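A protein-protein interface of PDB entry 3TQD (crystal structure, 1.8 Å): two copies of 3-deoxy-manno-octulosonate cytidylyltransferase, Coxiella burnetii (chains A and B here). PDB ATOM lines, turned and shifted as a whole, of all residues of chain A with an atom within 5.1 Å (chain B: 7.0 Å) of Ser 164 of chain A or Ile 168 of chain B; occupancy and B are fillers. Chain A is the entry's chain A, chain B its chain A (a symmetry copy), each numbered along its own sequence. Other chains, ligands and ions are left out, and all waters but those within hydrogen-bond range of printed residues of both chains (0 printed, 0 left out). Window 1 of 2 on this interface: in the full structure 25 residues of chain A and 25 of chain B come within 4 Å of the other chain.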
ATOM      1  N   SER A 149       7.598  12.463  -4.852  1.00  0.00           N
ATOM      2  CA  SER A 149       8.476  11.492  -5.533  1.00  0.00           C
ATOM      3  C   SER A 149       9.870  11.408  -4.903  1.00  0.00           C
ATOM      4  O   SER A 149      10.330  12.397  -4.351  1.00  0.00           O
ATOM      5  CB  SER A 149       8.604  11.804  -7.035  1.00  0.00           C
ATOM      6  OG  SER A 149       9.415  12.941  -7.316  1.00  0.00           O
ATOM      7  N   THR A 150      10.467  10.217  -4.873  1.00  0.00           N
ATOM      8  CA  THR A 150      11.826  10.077  -4.391  1.00  0.00           C
ATOM      9  C   THR A 150      12.795  10.035  -5.530  1.00  0.00           C
ATOM     10  O   THR A 150      12.705   9.177  -6.421  1.00  0.00           O
ATOM     11  CB  THR A 150      12.012   8.784  -3.544  1.00  0.00           C
ATOM     12  OG1 THR A 150      11.108   8.870  -2.475  1.00  0.00           O
ATOM     13  CG2 THR A 150      13.425   8.597  -2.971  1.00  0.00           C
ATOM     14  N   LYS A 151      13.771  10.939  -5.454  1.00  0.00           N
ATOM     15  CA  LYS A 151      14.841  11.004  -6.443  1.00  0.00           C
ATOM     16  C   LYS A 151      16.037  10.263  -5.911  1.00  0.00           C
ATOM     17  O   LYS A 151      16.232  10.171  -4.695  1.00  0.00           O
ATOM     18  CB  LYS A 151      15.204  12.455  -6.761  1.00  0.00           C
ATOM     19  CG  LYS A 151      14.394  13.162  -7.795  1.00  0.00           C
ATOM     20  CD  LYS A 151      12.894  13.385  -7.465  1.00  0.00           C
ATOM     21  CE  LYS A 151      12.599  14.105  -6.162  1.00  0.00           C
ATOM     22  NZ  LYS A 151      11.179  14.751  -6.126  1.00  0.00           N
ATOM     23  N   TYR A 162      22.828   9.339  -2.920  1.00  0.00           N
ATOM     24  CA  TYR A 162      21.803   9.912  -1.986  1.00  0.00           C
ATOM     25  C   TYR A 162      20.427   9.655  -2.512  1.00  0.00           C
ATOM     26  O   TYR A 162      20.255   9.497  -3.721  1.00  0.00           O
ATOM     27  CB  TYR A 162      22.114  11.406  -1.641  1.00  0.00           C
ATOM     28  CG  TYR A 162      21.271  11.969  -0.540  1.00  0.00           C
ATOM     29  CD1 TYR A 162      21.377  11.503   0.771  1.00  0.00           C
ATOM     30  CD2 TYR A 162      20.400  13.005  -0.788  1.00  0.00           C
ATOM     31  CE1 TYR A 162      20.533  11.983   1.783  1.00  0.00           C
ATOM     32  CE2 TYR A 162      19.616  13.548   0.242  1.00  0.00           C
ATOM     33  CZ  TYR A 162      19.666  13.024   1.498  1.00  0.00           C
ATOM     34  OH  TYR A 162      18.814  13.451   2.509  1.00  0.00           O
ATOM     35  N   PHE A 163      19.403   9.670  -1.593  1.00  0.00           N
ATOM     36  CA  PHE A 163      18.017   9.580  -1.959  1.00  0.00           C
ATOM     37  C   PHE A 163      17.350  10.767  -1.270  1.00  0.00           C
ATOM     38  O   PHE A 163      17.646  11.061  -0.091  1.00  0.00           O
ATOM     39  CB  PHE A 163      17.355   8.236  -1.466  1.00  0.00           C
ATOM     40  CG  PHE A 163      17.947   6.981  -1.990  1.00  0.00           C
ATOM     41  CD1 PHE A 163      17.261   6.214  -2.919  1.00  0.00           C
ATOM     42  CD2 PHE A 163      19.072   6.392  -1.354  1.00  0.00           C
ATOM     43  CE1 PHE A 163      17.757   4.988  -3.340  1.00  0.00           C
ATOM     44  CE2 PHE A 163      19.534   5.147  -1.748  1.00  0.00           C
ATOM     45  CZ  PHE A 163      18.922   4.483  -2.785  1.00  0.00           C
ATOM     46  N   SER A 164      16.402  11.401  -1.958  1.00  0.00           N
ATOM     47  CA  SER A 164      15.652  12.560  -1.419  1.00  0.00           C
ATOM     48  C   SER A 164      14.355  12.818  -2.100  1.00  0.00           C
ATOM     49  O   SER A 164      14.209  12.560  -3.319  1.00  0.00           O
ATOM     50  CB  SER A 164      16.488  13.861  -1.586  1.00  0.00           C
ATOM     51  OG  SER A 164      16.004  14.943  -0.863  1.00  0.00           O
ATOM     52  N   HIS A 165      13.479  13.503  -1.351  1.00  0.00           N
ATOM     53  CA  HIS A 165      12.301  14.153  -1.971  1.00  0.00           C
ATOM     54  C   HIS A 165      12.652  15.419  -2.688  1.00  0.00           C
ATOM     55  O   HIS A 165      11.898  15.885  -3.535  1.00  0.00           O
ATOM     56  CB  HIS A 165      11.174  14.390  -0.935  1.00  0.00           C
ATOM     57  CG  HIS A 165      10.662  13.142  -0.305  1.00  0.00           C
ATOM     58  ND1 HIS A 165       9.767  12.309  -0.944  1.00  0.00           N
ATOM     59  CD2 HIS A 165      10.998  12.517   0.848  1.00  0.00           C
ATOM     60  CE1 HIS A 165       9.548  11.243  -0.190  1.00  0.00           C
ATOM     61  NE2 HIS A 165      10.276  11.348   0.904  1.00  0.00           N
ATOM     62  N   ALA A 166      13.810  16.017  -2.382  1.00  0.00           N
ATOM     63  CA  ALA A 166      14.224  17.224  -3.073  1.00  0.00           C
ATOM     64  C   ALA A 166      14.624  16.955  -4.529  1.00  0.00           C
ATOM     65  O   ALA A 166      15.036  15.887  -4.854  1.00  0.00           O
ATOM     66  CB  ALA A 166      15.443  17.839  -2.349  1.00  0.00           C
ATOM     67  N   ILE A 168      16.935  16.616  -7.060  1.00  0.00           N
ATOM     68  CA  ILE A 168      18.364  16.410  -7.200  1.00  0.00           C
ATOM     69  C   ILE A 168      18.663  15.467  -8.344  1.00  0.00           C
ATOM     70  O   ILE A 168      17.929  14.493  -8.541  1.00  0.00           O
ATOM     71  CB  ILE A 168      19.029  15.934  -5.891  1.00  0.00           C
ATOM     72  CG1 ILE A 168      18.405  14.654  -5.385  1.00  0.00           C
ATOM     73  CG2 ILE A 168      18.927  17.069  -4.822  1.00  0.00           C
ATOM     74  CD1 ILE A 168      19.212  13.980  -4.222  1.00  0.00           C
ATOM     75  N   GLU A 216      13.528  12.784   5.894  1.00  0.00           N
ATOM     76  CA  GLU A 216      13.121  12.359   4.519  1.00  0.00           C
ATOM     77  C   GLU A 216      12.009  11.267   4.522  1.00  0.00           C
ATOM     78  O   GLU A 216      11.316  11.048   3.506  1.00  0.00           O
ATOM     79  CB  GLU A 216      14.323  11.826   3.751  1.00  0.00           C
ATOM     80  CG  GLU A 216      15.405  12.818   3.423  1.00  0.00           C
ATOM     81  CD  GLU A 216      15.279  13.513   2.091  1.00  0.00           C
ATOM     82  OE1 GLU A 216      14.242  13.384   1.401  1.00  0.00           O
ATOM     83  OE2 GLU A 216      16.268  14.169   1.685  1.00  0.00           O
ATOM     84  N   LEU A 218      12.851   8.178   4.602  1.00  0.00           N
ATOM     85  CA  LEU A 218      13.428   7.217   3.689  1.00  0.00           C
ATOM     86  C   LEU A 218      14.358   6.269   4.409  1.00  0.00           C
ATOM     87  O   LEU A 218      15.513   6.613   4.686  1.00  0.00           O
ATOM     88  CB  LEU A 218      14.162   7.980   2.568  1.00  0.00           C
ATOM     89  CG  LEU A 218      13.294   8.819   1.668  1.00  0.00           C
ATOM     90  CD1 LEU A 218      14.131   9.714   0.625  1.00  0.00           C
ATOM     91  CD2 LEU A 218      12.288   7.954   0.910  1.00  0.00           C
ATOM     92  N   ILE B 138      23.682  24.988   9.305  1.00  0.00           N
ATOM     93  CA  ILE B 138      22.638  25.903   8.871  1.00  0.00           C
ATOM     94  C   ILE B 138      21.595  25.946   9.980  1.00  0.00           C
ATOM     95  O   ILE B 138      21.026  24.961  10.326  1.00  0.00           O
ATOM     96  CB  ILE B 138      21.981  25.531   7.534  1.00  0.00           C
ATOM     97  CG1 ILE B 138      23.022  25.487   6.386  1.00  0.00           C
ATOM     98  CG2 ILE B 138      20.962  26.525   7.167  1.00  0.00           C
ATOM     99  CD1 ILE B 138      22.504  24.826   5.048  1.00  0.00           C
ATOM    100  N   LEU B 144      18.838  27.563   4.234  1.00  0.00           N
ATOM    101  CA  LEU B 144      18.573  26.234   3.733  1.00  0.00           C
ATOM    102  C   LEU B 144      17.904  26.237   2.371  1.00  0.00           C
ATOM    103  O   LEU B 144      18.312  25.522   1.432  1.00  0.00           O
ATOM    104  CB  LEU B 144      17.753  25.441   4.704  1.00  0.00           C
ATOM    105  CG  LEU B 144      17.324  24.056   4.288  1.00  0.00           C
ATOM    106  CD1 LEU B 144      18.551  23.129   3.870  1.00  0.00           C
ATOM    107  CD2 LEU B 144      16.567  23.343   5.422  1.00  0.00           C
ATOM    108  N   LYS B 151      24.409  22.893   0.145  1.00  0.00           N
ATOM    109  CA  LYS B 151      24.177  22.012   1.285  1.00  0.00           C
ATOM    110  C   LYS B 151      25.013  20.773   1.117  1.00  0.00           C
ATOM    111  O   LYS B 151      25.326  20.372  -0.009  1.00  0.00           O
ATOM    112  CB  LYS B 151      22.696  21.650   1.403  1.00  0.00           C
ATOM    113  CG  LYS B 151      21.806  22.598   2.131  1.00  0.00           C
ATOM    114  CD  LYS B 151      21.632  24.006   1.502  1.00  0.00           C
ATOM    115  CE  LYS B 151      21.156  24.036   0.061  1.00  0.00           C
ATOM    116  NZ  LYS B 151      20.513  25.399  -0.345  1.00  0.00           N
ATOM    117  N   VAL B 152      25.393  20.140   2.227  1.00  0.00           N
ATOM    118  CA  VAL B 152      26.092  18.891   2.188  1.00  0.00           C
ATOM    119  C   VAL B 152      25.434  17.976   3.220  1.00  0.00           C
ATOM    120  O   VAL B 152      24.959  18.447   4.312  1.00  0.00           O
ATOM    121  CB  VAL B 152      27.610  19.064   2.441  1.00  0.00           C
ATOM    122  CG1 VAL B 152      27.928  19.720   3.780  1.00  0.00           C
ATOM    123  CG2 VAL B 152      28.389  17.695   2.245  1.00  0.00           C
ATOM    124  N   VAL B 153      25.288  16.720   2.830  1.00  0.00           N
ATOM    125  CA  VAL B 153      24.715  15.669   3.694  1.00  0.00           C
ATOM    126  C   VAL B 153      25.819  14.735   4.064  1.00  0.00           C
ATOM    127  O   VAL B 153      26.651  14.317   3.219  1.00  0.00           O
ATOM    128  CB  VAL B 153      23.548  14.962   3.032  1.00  0.00           C
ATOM    129  CG1 VAL B 153      23.011  13.860   3.927  1.00  0.00           C
ATOM    130  CG2 VAL B 153      22.442  15.931   2.719  1.00  0.00           C
ATOM    131  N   TYR B 162      26.531  13.607  -0.385  1.00  0.00           N
ATOM    132  CA  TYR B 162      26.125  14.426  -1.576  1.00  0.00           C
ATOM    133  C   TYR B 162      26.270  15.883  -1.270  1.00  0.00           C
ATOM    134  O   TYR B 162      26.205  16.272  -0.104  1.00  0.00           O
ATOM    135  CB  TYR B 162      24.722  13.997  -2.116  1.00  0.00           C
ATOM    136  CG  TYR B 162      24.359  14.608  -3.434  1.00  0.00           C
ATOM    137  CD1 TYR B 162      25.056  14.292  -4.601  1.00  0.00           C
ATOM    138  CD2 TYR B 162      23.287  15.464  -3.534  1.00  0.00           C
ATOM    139  CE1 TYR B 162      24.759  14.924  -5.818  1.00  0.00           C
ATOM    140  CE2 TYR B 162      22.932  16.030  -4.768  1.00  0.00           C
ATOM    141  CZ  TYR B 162      23.674  15.783  -5.882  1.00  0.00           C
ATOM    142  OH  TYR B 162      23.429  16.424  -7.089  1.00  0.00           O
ATOM    143  N   PHE B 163      26.411  16.728  -2.347  1.00  0.00           N
ATOM    144  CA  PHE B 163      26.420  18.159  -2.228  1.00  0.00           C
ATOM    145  C   PHE B 163      25.371  18.644  -3.225  1.00  0.00           C
ATOM    146  O   PHE B 163      25.298  18.132  -4.364  1.00  0.00           O
ATOM    147  CB  PHE B 163      27.824  18.780  -2.588  1.00  0.00           C
ATOM    148  CG  PHE B 163      28.970  18.342  -1.753  1.00  0.00           C
ATOM    149  CD1 PHE B 163      29.549  19.214  -0.843  1.00  0.00           C
ATOM    150  CD2 PHE B 163      29.675  17.149  -2.061  1.00  0.00           C
ATOM    151  CE1 PHE B 163      30.684  18.852  -0.130  1.00  0.00           C
ATOM    152  CE2 PHE B 163      30.832  16.817  -1.377  1.00  0.00           C
ATOM    153  CZ  PHE B 163      31.292  17.629  -0.368  1.00  0.00           C
ATOM    154  N   SER B 164      24.613  19.670  -2.842  1.00  0.00           N
ATOM    155  CA  SER B 164      23.563  20.263  -3.704  1.00  0.00           C
ATOM    156  C   SER B 164      23.174  21.648  -3.325  1.00  0.00           C
ATOM    157  O   SER B 164      23.205  22.018  -2.126  1.00  0.00           O
ATOM    158  CB  SER B 164      22.262  19.416  -3.620  1.00  0.00           C
ATOM    159  OG  SER B 164      21.324  19.719  -4.598  1.00  0.00           O
ATOM    160  N   HIS B 165      22.627  22.349  -4.329  1.00  0.00           N
ATOM    161  CA  HIS B 165      21.864  23.589  -4.056  1.00  0.00           C
ATOM    162  C   HIS B 165      20.492  23.316  -3.522  1.00  0.00           C
ATOM    163  O   HIS B 165      19.873  24.187  -2.922  1.00  0.00           O
ATOM    164  CB  HIS B 165      21.807  24.505  -5.305  1.00  0.00           C
ATOM    165  CG  HIS B 165      23.143  24.950  -5.787  1.00  0.00           C
ATOM    166  ND1 HIS B 165      23.838  25.978  -5.184  1.00  0.00           N
ATOM    167  CD2 HIS B 165      23.970  24.443  -6.732  1.00  0.00           C
ATOM    168  CE1 HIS B 165      25.021  26.106  -5.765  1.00  0.00           C
ATOM    169  NE2 HIS B 165      25.123  25.192  -6.711  1.00  0.00           N
ATOM    170  N   ALA B 166      19.972  22.099  -3.715  1.00  0.00           N
ATOM    171  CA  ALA B 166      18.664  21.763  -3.183  1.00  0.00           C
ATOM    172  C   ALA B 166      18.668  21.637  -1.656  1.00  0.00           C
ATOM    173  O   ALA B 166      19.664  21.335  -1.078  1.00  0.00           O
ATOM    174  CB  ALA B 166      18.201  20.409  -3.772  1.00  0.00           C
ATOM    175  N   PRO B 167      17.514  21.857  -1.016  1.00  0.00           N
ATOM    176  CA  PRO B 167      17.431  21.746   0.434  1.00  0.00           C
ATOM    177  C   PRO B 167      17.379  20.325   0.952  1.00  0.00           C
ATOM    178  O   PRO B 167      16.325  19.702   1.041  1.00  0.00           O
ATOM    179  CB  PRO B 167      16.191  22.620   0.787  1.00  0.00           C
ATOM    180  CG  PRO B 167      15.426  22.638  -0.407  1.00  0.00           C
ATOM    181  CD  PRO B 167      16.326  22.519  -1.593  1.00  0.00           C
ATOM    182  N   ILE B 168      18.567  19.824   1.272  1.00  0.00           N
ATOM    183  CA  ILE B 168      18.758  18.452   1.702  1.00  0.00           C
ATOM    184  C   ILE B 168      19.481  18.400   3.029  1.00  0.00           C
ATOM    185  O   ILE B 168      20.396  19.198   3.258  1.00  0.00           O
ATOM    186  CB  ILE B 168      19.469  17.588   0.639  1.00  0.00           C
ATOM    187  CG1 ILE B 168      20.813  18.166   0.263  1.00  0.00           C
ATOM    188  CG2 ILE B 168      18.545  17.452  -0.613  1.00  0.00           C
ATOM    189  CD1 ILE B 168      21.695  17.196  -0.597  1.00  0.00           C
ATOM    190  N   PRO B 169      19.088  17.455   3.892  1.00  0.00           N
ATOM    191  CA  PRO B 169      17.995  16.547   3.729  1.00  0.00           C
ATOM    192  C   PRO B 169      16.645  17.246   3.730  1.00  0.00           C
ATOM    193  O   PRO B 169      16.420  18.270   4.427  1.00  0.00           O
ATOM    194  CB  PRO B 169      18.105  15.608   4.931  1.00  0.00           C
ATOM    195  CG  PRO B 169      19.459  15.779   5.404  1.00  0.00           C
ATOM    196  CD  PRO B 169      19.857  17.149   5.117  1.00  0.00           C
ATOM    197  N   TRP B 170      15.755  16.707   2.932  1.00  0.00           N
ATOM    198  CA  TRP B 170      14.387  17.266   2.834  1.00  0.00           C
ATOM    199  C   TRP B 170      13.507  16.769   3.972  1.00  0.00           C
ATOM    200  O   TRP B 170      13.513  15.571   4.283  1.00  0.00           O
ATOM    201  CB  TRP B 170      13.832  16.865   1.443  1.00  0.00           C
ATOM    202  CG  TRP B 170      12.443  17.389   1.191  1.00  0.00           C
ATOM    203  CD1 TRP B 170      11.285  16.867   1.588  1.00  0.00           C
ATOM    204  CD2 TRP B 170      12.133  18.573   0.461  1.00  0.00           C
ATOM    205  NE1 TRP B 170      10.219  17.645   1.140  1.00  0.00           N
ATOM    206  CE2 TRP B 170      10.725  18.707   0.450  1.00  0.00           C
ATOM    207  CE3 TRP B 170      12.913  19.514  -0.185  1.00  0.00           C
ATOM    208  CZ2 TRP B 170      10.080  19.737  -0.208  1.00  0.00           C
ATOM    209  CZ3 TRP B 170      12.288  20.531  -0.864  1.00  0.00           C
ATOM    210  CH2 TRP B 170      10.871  20.673  -0.825  1.00  0.00           C
ATOM    211  N   GLY B 171      12.726  17.681   4.578  1.00  0.00           N
ATOM    212  CA  GLY B 171      11.786  17.324   5.662  1.00  0.00           C
ATOM    213  C   GLY B 171      10.465  17.023   5.033  1.00  0.00           C
ATOM    214  O   GLY B 171       9.748  17.963   4.707  1.00  0.00           O
ATOM    215  N   PHE B 175       8.687  20.452   5.689  1.00  0.00           N
ATOM    216  CA  PHE B 175       9.014  21.556   4.751  1.00  0.00           C
ATOM    217  C   PHE B 175       7.794  22.273   4.202  1.00  0.00           C
ATOM    218  O   PHE B 175       7.911  23.381   3.637  1.00  0.00           O
ATOM    219  CB  PHE B 175       9.905  21.013   3.605  1.00  0.00           C
ATOM    220  CG  PHE B 175      11.345  20.929   3.944  1.00  0.00           C
ATOM    221  CD1 PHE B 175      11.804  20.857   5.257  1.00  0.00           C
ATOM    222  CD2 PHE B 175      12.301  20.801   2.902  1.00  0.00           C
ATOM    223  CE1 PHE B 175      13.143  20.796   5.555  1.00  0.00           C
ATOM    224  CE2 PHE B 175      13.661  20.737   3.204  1.00  0.00           C
ATOM    225  CZ  PHE B 175      14.103  20.703   4.524  1.00  0.00           C
ATOM    226  N   SER B 186      20.759  19.690  11.915  1.00  0.00           N
ATOM    227  CA  SER B 186      20.136  18.933  10.876  1.00  0.00           C
ATOM    228  C   SER B 186      20.754  19.140   9.448  1.00  0.00           C
ATOM    229  O   SER B 186      20.656  18.270   8.591  1.00  0.00           O
ATOM    230  CB  SER B 186      18.613  19.222  10.906  1.00  0.00           C
ATOM    231  OG  SER B 186      18.308  20.628  10.883  1.00  0.00           O
ATOM    232  N   HIS B 187      21.430  20.249   9.237  1.00  0.00           N
ATOM    233  CA  HIS B 187      21.763  20.751   7.935  1.00  0.00           C
ATOM    234  C   HIS B 187      23.079  21.518   8.017  1.00  0.00           C
ATOM    235  O   HIS B 187      23.336  22.207   9.030  1.00  0.00           O
ATOM    236  CB  HIS B 187      20.667  21.676   7.411  1.00  0.00           C
ATOM    237  CG  HIS B 187      19.365  20.993   7.140  1.00  0.00           C
ATOM    238  ND1 HIS B 187      18.385  20.829   8.119  1.00  0.00           N
ATOM    239  CD2 HIS B 187      18.877  20.436   6.004  1.00  0.00           C
ATOM    240  CE1 HIS B 187      17.384  20.133   7.590  1.00  0.00           C
ATOM    241  NE2 HIS B 187      17.651  19.892   6.312  1.00  0.00           N
ATOM    242  N   TYR B 188      23.866  21.408   6.950  1.00  0.00           N
ATOM    243  CA  TYR B 188      25.221  21.902   6.866  1.00  0.00           C
ATOM    244  C   TYR B 188      25.430  22.588   5.540  1.00  0.00           C
ATOM    245  O   TYR B 188      24.999  22.104   4.465  1.00  0.00           O
ATOM    246  CB  TYR B 188      26.261  20.757   6.995  1.00  0.00           C
ATOM    247  CG  TYR B 188      26.213  20.110   8.347  1.00  0.00           C
ATOM    248  CD1 TYR B 188      26.904  20.676   9.414  1.00  0.00           C
ATOM    249  CD2 TYR B 188      25.450  18.954   8.600  1.00  0.00           C
ATOM    250  CE1 TYR B 188      26.871  20.114  10.676  1.00  0.00           C
ATOM    251  CE2 TYR B 188      25.433  18.397   9.844  1.00  0.00           C
ATOM    252  CZ  TYR B 188      26.146  18.979  10.876  1.00  0.00           C
ATOM    253  OH  TYR B 188      26.134  18.469  12.153  1.00  0.00           O
ATOM    254  N   GLU B 216      24.646  21.054 -11.204  1.00  0.00           N
ATOM    255  CA  GLU B 216      24.810  21.715  -9.872  1.00  0.00           C
ATOM    256  C   GLU B 216      25.874  22.855  -9.883  1.00  0.00           C
ATOM    257  O   GLU B 216      25.899  23.724  -8.988  1.00  0.00           O
ATOM    258  CB  GLU B 216      25.208  20.690  -8.817  1.00  0.00           C
ATOM    259  CG  GLU B 216      24.184  19.643  -8.479  1.00  0.00           C
ATOM    260  CD  GLU B 216      23.258  19.972  -7.335  1.00  0.00           C
ATOM    261  OE1 GLU B 216      23.250  21.118  -6.833  1.00  0.00           O
ATOM    262  OE2 GLU B 216      22.549  19.043  -6.879  1.00  0.00           O
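The side-chain carboxylate (OE2) of Glu 216 of chain A lies within hydrogen-bond range of the backbone NH (N) of Trp 170 of chain B, 2.9 Å away.
The backbone carbonyl oxygen (O) of Ser 164 of chain B lies within hydrogen-bond range of the backbone NH (N) of Lys 151 of chain B, at 2.7 Å. The side-chain amino group (NZ) of Lys 151 of chain A is in hydrogen-bond range of the backbone carbonyl oxygen (O) of His 165 of chain A (2.9 Å). The side-chain carboxylate (OE2) of Glu 216 of chain A sits at hydrogen-bond distance from the side-chain hydroxyl (OG) of Ser 164 of chain A (2.7 Å). The backbone carbonyl oxygen (O) of Pro 169 of chain B sits at hydrogen-bond distance from a ring nitrogen (NE2) of His 187 of chain B (2.8 Å). The side-chain hydroxyl (OG) of Ser 164 of chain B sits at hydrogen-bond distance from the backbone NH (N) of Ala 166 of chain B (2.9 Å). The backbone carbonyl oxygen of Ser 149 of chain A is in hydrogen-bond range of a ring nitrogen (ND1) of His 165 of chain A, at 3.5 Å.
Val 153 of chain B touches Tyr 162 of chain A. CB of Tyr 162 of chain B touches CB of Tyr 162 of chain A (3.7 Å). Tyr 162 of chain A touches Pro 169 of chain B. Ser 164 of chain A touches Ile 168 of chain B. Ser 164 of chain A touches Trp 170 of chain B. His 165 of chain A touches Trp 170 of chain B (CB to CD1, 3.5 Å). CB of Ala 166 of chain A touches O of Pro 167 of chain B (3.97 Å). Ala 166 of chain A touches Ile 168 of chain B. Ala 166 of chain A touches Trp 170 of chain B (CB to CE3, 3.7 Å). Ser 164 of chain B touches Ile 168 of chain A.
Of chain B, only Ile 168 (3.6 Å) and Trp 170 (3.7 Å) come within 4 Å of Ser 164 of chain A. Of the printed residues of chain B, His 165 of chain A touches Trp 170. Phe 163 of chain B touches none of the printed residues of chain A. Printed residues of chain A within 4 Å of Ala 166 of chain B: Ile 168. Of the printed residues of chain A, Ile 168 of chain B touches Ser 164 (3.6 Å) and Ala 166 (3.6 Å). Of the printed residues of chain A, Trp 170 of chain B touches Ser 164, His 165, Ala 166 and Glu 216.
Hydrophobic or aromatic side chains of chain A that line the printed part of chain B: Tyr 162, His 165, Ala 166 and Ile 168. Among the printed residues, no Asp or Glu carboxylate lies within 4 Å of a Lys or Arg side-chain nitrogen of the other chain.
Tyr 162 of chain B touches its own counterpart, Tyr 162 of chain A. Ser 164 of chain A touches Ile 168 of chain B, and with the chains exchanged Ile 168 of chain A touches Ser 164 of chain B. Ala 166 of chain A touches Ile 168 of chain B, and with the chains exchanged Ile 168 of chain A touches Ala 166 of chain B. Of the 13 pairs that touch across the chains among the printed residues, 5 have their exchanged pair printed and touching as well.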
